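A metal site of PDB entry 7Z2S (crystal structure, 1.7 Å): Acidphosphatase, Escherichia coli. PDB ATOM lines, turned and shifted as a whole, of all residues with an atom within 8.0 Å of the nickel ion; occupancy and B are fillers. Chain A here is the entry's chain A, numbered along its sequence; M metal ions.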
ATOM      1  N   ARG A  18     -27.869   0.117 -13.489  1.00  0.00           N
ATOM      2  CA  ARG A  18     -26.635  -0.145 -14.200  1.00  0.00           C
ATOM      3  C   ARG A  18     -26.958  -0.346 -15.670  1.00  0.00           C
ATOM      4  O   ARG A  18     -28.042  -0.832 -16.025  1.00  0.00           O
ATOM      5  CB  ARG A  18     -25.916  -1.381 -13.620  1.00  0.00           C
ATOM      6  CG  ARG A  18     -24.559  -1.611 -14.265  1.00  0.00           C
ATOM      7  CD  ARG A  18     -23.877  -2.869 -13.790  1.00  0.00           C
ATOM      8  NE  ARG A  18     -22.674  -3.067 -14.590  1.00  0.00           N
ATOM      9  CZ  ARG A  18     -22.055  -4.225 -14.737  1.00  0.00           C
ATOM     10  NH1 ARG A  18     -22.518  -5.338 -14.188  1.00  0.00           N
ATOM     11  NH2 ARG A  18     -20.922  -4.269 -15.435  1.00  0.00           N
ATOM     12  N   ARG A  22     -22.469  -5.192 -21.868  1.00  0.00           N
ATOM     13  CA  ARG A  22     -21.530  -4.472 -22.711  1.00  0.00           C
ATOM     14  C   ARG A  22     -20.331  -5.359 -22.995  1.00  0.00           C
ATOM     15  O   ARG A  22     -20.036  -6.299 -22.249  1.00  0.00           O
ATOM     16  CB  ARG A  22     -21.035  -3.186 -22.031  1.00  0.00           C
ATOM     17  CG  ARG A  22     -20.478  -3.471 -20.641  1.00  0.00           C
ATOM     18  CD  ARG A  22     -19.325  -2.563 -20.261  1.00  0.00           C
ATOM     19  NE  ARG A  22     -18.868  -2.831 -18.917  1.00  0.00           N
ATOM     20  CZ  ARG A  22     -18.008  -3.796 -18.606  1.00  0.00           C
ATOM     21  NH1 ARG A  22     -17.509  -4.592 -19.540  1.00  0.00           N
ATOM     22  NH2 ARG A  22     -17.646  -3.971 -17.331  1.00  0.00           N
ATOM     23  N   SER A 217     -11.468  -9.296 -10.244  1.00  0.00           N
ATOM     24  CA  SER A 217     -12.771  -8.656 -10.313  1.00  0.00           C
ATOM     25  C   SER A 217     -13.197  -8.446 -11.762  1.00  0.00           C
ATOM     26  O   SER A 217     -14.352  -8.718 -12.119  1.00  0.00           O
ATOM     27  CB  SER A 217     -12.733  -7.323  -9.569  1.00  0.00           C
ATOM     28  OG  SER A 217     -13.970  -6.664  -9.682  1.00  0.00           O
ATOM     29  N   GLU A 221     -16.206 -10.775 -13.833  1.00  0.00           N
ATOM     30  CA  GLU A 221     -17.255  -9.998 -14.502  1.00  0.00           C
ATOM     31  C   GLU A 221     -17.359 -10.373 -15.971  1.00  0.00           C
ATOM     32  O   GLU A 221     -18.466 -10.509 -16.503  1.00  0.00           O
ATOM     33  CB  GLU A 221     -16.933  -8.503 -14.356  1.00  0.00           C
ATOM     34  CG  GLU A 221     -17.944  -7.468 -14.904  1.00  0.00           C
ATOM     35  CD  GLU A 221     -19.361  -7.598 -14.347  1.00  0.00           C
ATOM     36  OE1 GLU A 221     -19.557  -8.329 -13.338  1.00  0.00           O
ATOM     37  OE2 GLU A 221     -20.268  -6.902 -14.870  1.00  0.00           O
ATOM     38  N   LEU A 224     -19.228 -13.593 -16.503  1.00  0.00           N
ATOM     39  CA  LEU A 224     -20.653 -13.369 -16.322  1.00  0.00           C
ATOM     40  C   LEU A 224     -21.258 -12.695 -17.550  1.00  0.00           C
ATOM     41  O   LEU A 224     -22.368 -13.032 -17.959  1.00  0.00           O
ATOM     42  CB  LEU A 224     -20.908 -12.544 -15.073  1.00  0.00           C
ATOM     43  CG  LEU A 224     -22.382 -12.427 -14.690  1.00  0.00           C
ATOM     44  CD1 LEU A 224     -22.657 -12.931 -13.271  1.00  0.00           C
ATOM     45  CD2 LEU A 224     -22.819 -10.982 -14.839  1.00  0.00           C
ATOM     46  N   LEU A 249     -17.763 -14.880  -8.885  1.00  0.00           N
ATOM     47  CA  LEU A 249     -18.168 -13.485  -8.804  1.00  0.00           C
ATOM     48  C   LEU A 249     -17.996 -12.914  -7.409  1.00  0.00           C
ATOM     49  O   LEU A 249     -18.050 -11.690  -7.248  1.00  0.00           O
ATOM     50  CB  LEU A 249     -19.621 -13.330  -9.270  1.00  0.00           C
ATOM     51  CG  LEU A 249     -19.804 -13.079 -10.778  1.00  0.00           C
ATOM     52  CD1 LEU A 249     -19.168 -11.745 -11.225  1.00  0.00           C
ATOM     53  CD2 LEU A 249     -19.254 -14.252 -11.601  1.00  0.00           C
ATOM     54  N   HIS A 252     -15.434 -10.259  -7.747  1.00  0.00           N
ATOM     55  CA  HIS A 252     -15.979  -8.995  -8.224  1.00  0.00           C
ATOM     56  C   HIS A 252     -16.716  -8.278  -7.096  1.00  0.00           C
ATOM     57  O   HIS A 252     -16.498  -7.080  -6.845  1.00  0.00           O
ATOM     58  CB  HIS A 252     -16.911  -9.258  -9.411  1.00  0.00           C
ATOM     59  CG  HIS A 252     -17.711  -8.064  -9.858  1.00  0.00           C
ATOM     60  ND1 HIS A 252     -17.170  -7.040 -10.613  1.00  0.00           N
ATOM     61  CD2 HIS A 252     -19.025  -7.754  -9.697  1.00  0.00           C
ATOM     62  CE1 HIS A 252     -18.114  -6.150 -10.891  1.00  0.00           C
ATOM     63  NE2 HIS A 252     -19.250  -6.562 -10.347  1.00  0.00           N
ATOM     64  N   ASN A 253     -17.592  -8.996  -6.386  1.00  0.00           N
ATOM     65  CA  ASN A 253     -18.339  -8.373  -5.305  1.00  0.00           C
ATOM     66  C   ASN A 253     -17.421  -7.877  -4.205  1.00  0.00           C
ATOM     67  O   ASN A 253     -17.655  -6.813  -3.614  1.00  0.00           O
ATOM     68  CB  ASN A 253     -19.366  -9.351  -4.732  1.00  0.00           C
ATOM     69  CG  ASN A 253     -20.393  -9.738  -5.753  1.00  0.00           C
ATOM     70  OD1 ASN A 253     -20.733  -8.935  -6.628  1.00  0.00           O
ATOM     71  ND2 ASN A 253     -20.894 -10.975  -5.667  1.00  0.00           N
ATOM     72  N   PHE A 256     -15.815  -4.512  -5.064  1.00  0.00           N
ATOM     73  CA  PHE A 256     -16.708  -3.362  -4.965  1.00  0.00           C
ATOM     74  C   PHE A 256     -17.062  -3.072  -3.515  1.00  0.00           C
ATOM     75  O   PHE A 256     -17.295  -1.904  -3.153  1.00  0.00           O
ATOM     76  CB  PHE A 256     -17.964  -3.581  -5.816  1.00  0.00           C
ATOM     77  CG  PHE A 256     -17.783  -3.181  -7.251  1.00  0.00           C
ATOM     78  CD1 PHE A 256     -17.027  -3.952  -8.110  1.00  0.00           C
ATOM     79  CD2 PHE A 256     -18.301  -1.984  -7.720  1.00  0.00           C
ATOM     80  CE1 PHE A 256     -16.825  -3.578  -9.420  1.00  0.00           C
ATOM     81  CE2 PHE A 256     -18.097  -1.596  -9.030  1.00  0.00           C
ATOM     82  CZ  PHE A 256     -17.357  -2.393  -9.890  1.00  0.00           C
ATOM     83  N   HIS A 305     -23.759   3.175 -13.705  1.00  0.00           N
ATOM     84  CA  HIS A 305     -22.695   2.167 -13.697  1.00  0.00           C
ATOM     85  C   HIS A 305     -22.739   1.347 -12.409  1.00  0.00           C
ATOM     86  O   HIS A 305     -23.420   1.694 -11.443  1.00  0.00           O
ATOM     87  CB  HIS A 305     -21.314   2.820 -13.826  1.00  0.00           C
ATOM     88  CG  HIS A 305     -21.204   3.737 -15.000  1.00  0.00           C
ATOM     89  ND1 HIS A 305     -20.822   3.311 -16.245  1.00  0.00           N
ATOM     90  CD2 HIS A 305     -21.421   5.081 -15.111  1.00  0.00           C
ATOM     91  CE1 HIS A 305     -20.822   4.327 -17.086  1.00  0.00           C
ATOM     92  NE2 HIS A 305     -21.174   5.415 -16.412  1.00  0.00           N
ATOM     93  N   ASP A 306     -21.993   0.243 -12.460  1.00  0.00           N
ATOM     94  CA  ASP A 306     -21.838  -0.663 -11.321  1.00  0.00           C
ATOM     95  C   ASP A 306     -21.500   0.098 -10.045  1.00  0.00           C
ATOM     96  O   ASP A 306     -22.119  -0.099  -8.997  1.00  0.00           O
ATOM     97  CB  ASP A 306     -20.755  -1.683 -11.694  1.00  0.00           C
ATOM     98  CG  ASP A 306     -20.754  -2.897 -10.801  1.00  0.00           C
ATOM     99  OD1 ASP A 306     -20.731  -2.729  -9.564  1.00  0.00           O
ATOM    100  OD2 ASP A 306     -20.808  -4.026 -11.337  1.00  0.00           O
ATOM    101  N   THR A 307     -20.508   1.002 -10.133  1.00  0.00           N
ATOM    102  CA  THR A 307     -20.078   1.789  -8.977  1.00  0.00           C
ATOM    103  C   THR A 307     -21.200   2.665  -8.439  1.00  0.00           C
ATOM    104  O   THR A 307     -21.294   2.851  -7.230  1.00  0.00           O
ATOM    105  CB  THR A 307     -18.839   2.635  -9.280  1.00  0.00           C
ATOM    106  OG1 THR A 307     -19.194   3.779 -10.057  1.00  0.00           O
ATOM    107  CG2 THR A 307     -17.700   1.865  -9.954  1.00  0.00           C
ATOM    108  N   LEU A 309     -24.464   1.999  -8.219  1.00  0.00           N
ATOM    109  CA  LEU A 309     -25.263   1.166  -7.330  1.00  0.00           C
ATOM    110  C   LEU A 309     -24.541   0.910  -6.019  1.00  0.00           C
ATOM    111  O   LEU A 309     -25.125   1.031  -4.935  1.00  0.00           O
ATOM    112  CB  LEU A 309     -25.619  -0.164  -8.007  1.00  0.00           C
ATOM    113  CG  LEU A 309     -26.524  -0.154  -9.227  1.00  0.00           C
ATOM    114  CD1 LEU A 309     -26.873  -1.571  -9.625  1.00  0.00           C
ATOM    115  CD2 LEU A 309     -27.798   0.581  -8.884  1.00  0.00           C
ATOM    116  N   ALA A 310     -23.270   0.530  -6.091  1.00  0.00           N
ATOM    117  CA  ALA A 310     -22.516   0.245  -4.866  1.00  0.00           C
ATOM    118  C   ALA A 310     -22.369   1.493  -4.000  1.00  0.00           C
ATOM    119  O   ALA A 310     -22.499   1.420  -2.770  1.00  0.00           O
ATOM    120  CB  ALA A 310     -21.155  -0.357  -5.225  1.00  0.00           C
ATOM    121  N   GLN A 325     -28.396 -14.451  -8.875  1.00  0.00           N
ATOM    122  CA  GLN A 325     -27.575 -13.530  -9.655  1.00  0.00           C
ATOM    123  C   GLN A 325     -26.250 -13.367  -8.923  1.00  0.00           C
ATOM    124  O   GLN A 325     -26.189 -12.631  -7.927  1.00  0.00           O
ATOM    125  CB  GLN A 325     -28.290 -12.199  -9.857  1.00  0.00           C
ATOM    126  CG  GLN A 325     -27.473 -11.125 -10.546  1.00  0.00           C
ATOM    127  CD  GLN A 325     -26.810 -11.640 -11.807  1.00  0.00           C
ATOM    128  OE1 GLN A 325     -25.627 -11.965 -11.824  1.00  0.00           O
ATOM    129  NE2 GLN A 325     -27.582 -11.731 -12.881  1.00  0.00           N
ATOM    130  N   PRO A 326     -25.183 -14.026  -9.371  1.00  0.00           N
ATOM    131  CA  PRO A 326     -23.916 -13.984  -8.619  1.00  0.00           C
ATOM    132  C   PRO A 326     -23.300 -12.608  -8.505  1.00  0.00           C
ATOM    133  O   PRO A 326     -22.519 -12.354  -7.571  1.00  0.00           O
ATOM    134  CB  PRO A 326     -23.003 -14.940  -9.404  1.00  0.00           C
ATOM    135  CG  PRO A 326     -23.865 -15.683 -10.330  1.00  0.00           C
ATOM    136  CD  PRO A 326     -25.085 -14.854 -10.581  1.00  0.00           C
ATOM    137  N   ASP A 327     -23.583 -11.708  -9.459  1.00  0.00           N
ATOM    138  CA  ASP A 327     -23.045 -10.351  -9.466  1.00  0.00           C
ATOM    139  C   ASP A 327     -23.999  -9.455  -8.693  1.00  0.00           C
ATOM    140  O   ASP A 327     -25.122  -9.200  -9.129  1.00  0.00           O
ATOM    141  CB  ASP A 327     -22.863  -9.888 -10.915  1.00  0.00           C
ATOM    142  CG  ASP A 327     -22.296  -8.476 -11.033  1.00  0.00           C
ATOM    143  OD1 ASP A 327     -22.139  -7.764 -10.022  1.00  0.00           O
ATOM    144  OD2 ASP A 327     -22.026  -8.044 -12.174  1.00  0.00           O
ATOM    145  N   ASN A 328     -23.549  -8.962  -7.537  1.00  0.00           N
ATOM    146  CA  ASN A 328     -24.404  -8.131  -6.696  1.00  0.00           C
ATOM    147  C   ASN A 328     -24.723  -6.792  -7.338  1.00  0.00           C
ATOM    148  O   ASN A 328     -25.604  -6.067  -6.838  1.00  0.00           O
ATOM    149  CB  ASN A 328     -23.739  -7.923  -5.351  1.00  0.00           C
ATOM    150  CG  ASN A 328     -24.017  -9.054  -4.411  1.00  0.00           C
ATOM    151  OD1 ASN A 328     -23.312  -9.252  -3.430  1.00  0.00           O
ATOM    152  ND2 ASN A 328     -25.022  -9.861  -4.745  1.00  0.00           N
ATOM    153  N   THR A 329     -24.031  -6.427  -8.416  1.00  0.00           N
ATOM    154  CA  THR A 329     -24.295  -5.207  -9.175  1.00  0.00           C
ATOM    155  C   THR A 329     -24.356  -5.601 -10.656  1.00  0.00           C
ATOM    156  O   THR A 329     -23.449  -5.295 -11.428  1.00  0.00           O
ATOM    157  CB  THR A 329     -23.233  -4.144  -8.898  1.00  0.00           C
ATOM    158  OG1 THR A 329     -21.922  -4.744  -8.860  1.00  0.00           O
ATOM    159  CG2 THR A 329     -23.463  -3.488  -7.544  1.00  0.00           C
ATOM    160  N   PRO A 330     -25.417  -6.285 -11.067  1.00  0.00           N
ATOM    161  CA  PRO A 330     -25.420  -6.963 -12.362  1.00  0.00           C
ATOM    162  C   PRO A 330     -25.834  -6.012 -13.469  1.00  0.00           C
ATOM    163  O   PRO A 330     -26.445  -4.971 -13.213  1.00  0.00           O
ATOM    164  CB  PRO A 330     -26.455  -8.078 -12.176  1.00  0.00           C
ATOM    165  CG  PRO A 330     -27.463  -7.468 -11.232  1.00  0.00           C
ATOM    166  CD  PRO A 330     -26.677  -6.518 -10.329  1.00  0.00           C
ATOM    167  N   PRO A 331     -25.513  -6.346 -14.719  1.00  0.00           N
ATOM    168  CA  PRO A 331     -26.026  -5.557 -15.850  1.00  0.00           C
ATOM    169  C   PRO A 331     -27.533  -5.399 -15.747  1.00  0.00           C
ATOM    170  O   PRO A 331     -28.266  -6.353 -15.499  1.00  0.00           O
ATOM    171  CB  PRO A 331     -25.626  -6.390 -17.069  1.00  0.00           C
ATOM    172  CG  PRO A 331     -24.447  -7.226 -16.590  1.00  0.00           C
ATOM    173  CD  PRO A 331     -24.731  -7.514 -15.155  1.00  0.00           C
HETATM  174 NI    NI M   1     -21.302  -5.862 -10.799  1.00  0.00          NI
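The side-chain carboxylate (OD2) of Asp 306 lies close to the guanidinium group (NH1) of Arg 18 (3.6 Å).
A ring nitrogen (NE2) of His 252 sits close to the side-chain carboxylate (OE1) of Glu 221 (3.5 Å).
OG of Ser 217 is in hydrogen-bond range of ND1 of His 252.
The side-chain carboxylate (OD2) of Asp 327 is in salt-bridge range of the guanidinium group (NH1) of Arg 18.
The side-chain carboxylate (OD2) of Asp 327 sits close to the side-chain carboxylate (OE1) of Glu 221, at 2.7 Å.
The backbone NH of Asp 327 is in hydrogen-bond range of the side-chain amide oxygen of Gln 325.
O of Thr 329 sits close to NH1 of Arg 18 (2.9 Å).
OE2 of Glu 221 is in salt-bridge range of NH2 of Arg 18 (2.8 Å).
Arg 18 touches the nickel ion (NH1 to NI, 3.6 Å).
Glu 221 touches the nickel ion.
The nearest printed residue that does not touch the nickel ion is Pro 330 (4.1 Å).
The nickel ion is bound by the side-chain carboxylate (OD2) of Asp 306, a ring nitrogen (NE2) of His 252, the side-chain carboxylate (OD1) of Asp 327, the backbone carbonyl oxygen (O) of Thr 329 and the side-chain hydroxyl (OG1) of Thr 329.
The nickel ion has five donor atoms within binding distance.
Slightly farther from the nickel ion lies the side-chain carboxylate (OD2) of Asp 327 (2.7 Å).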
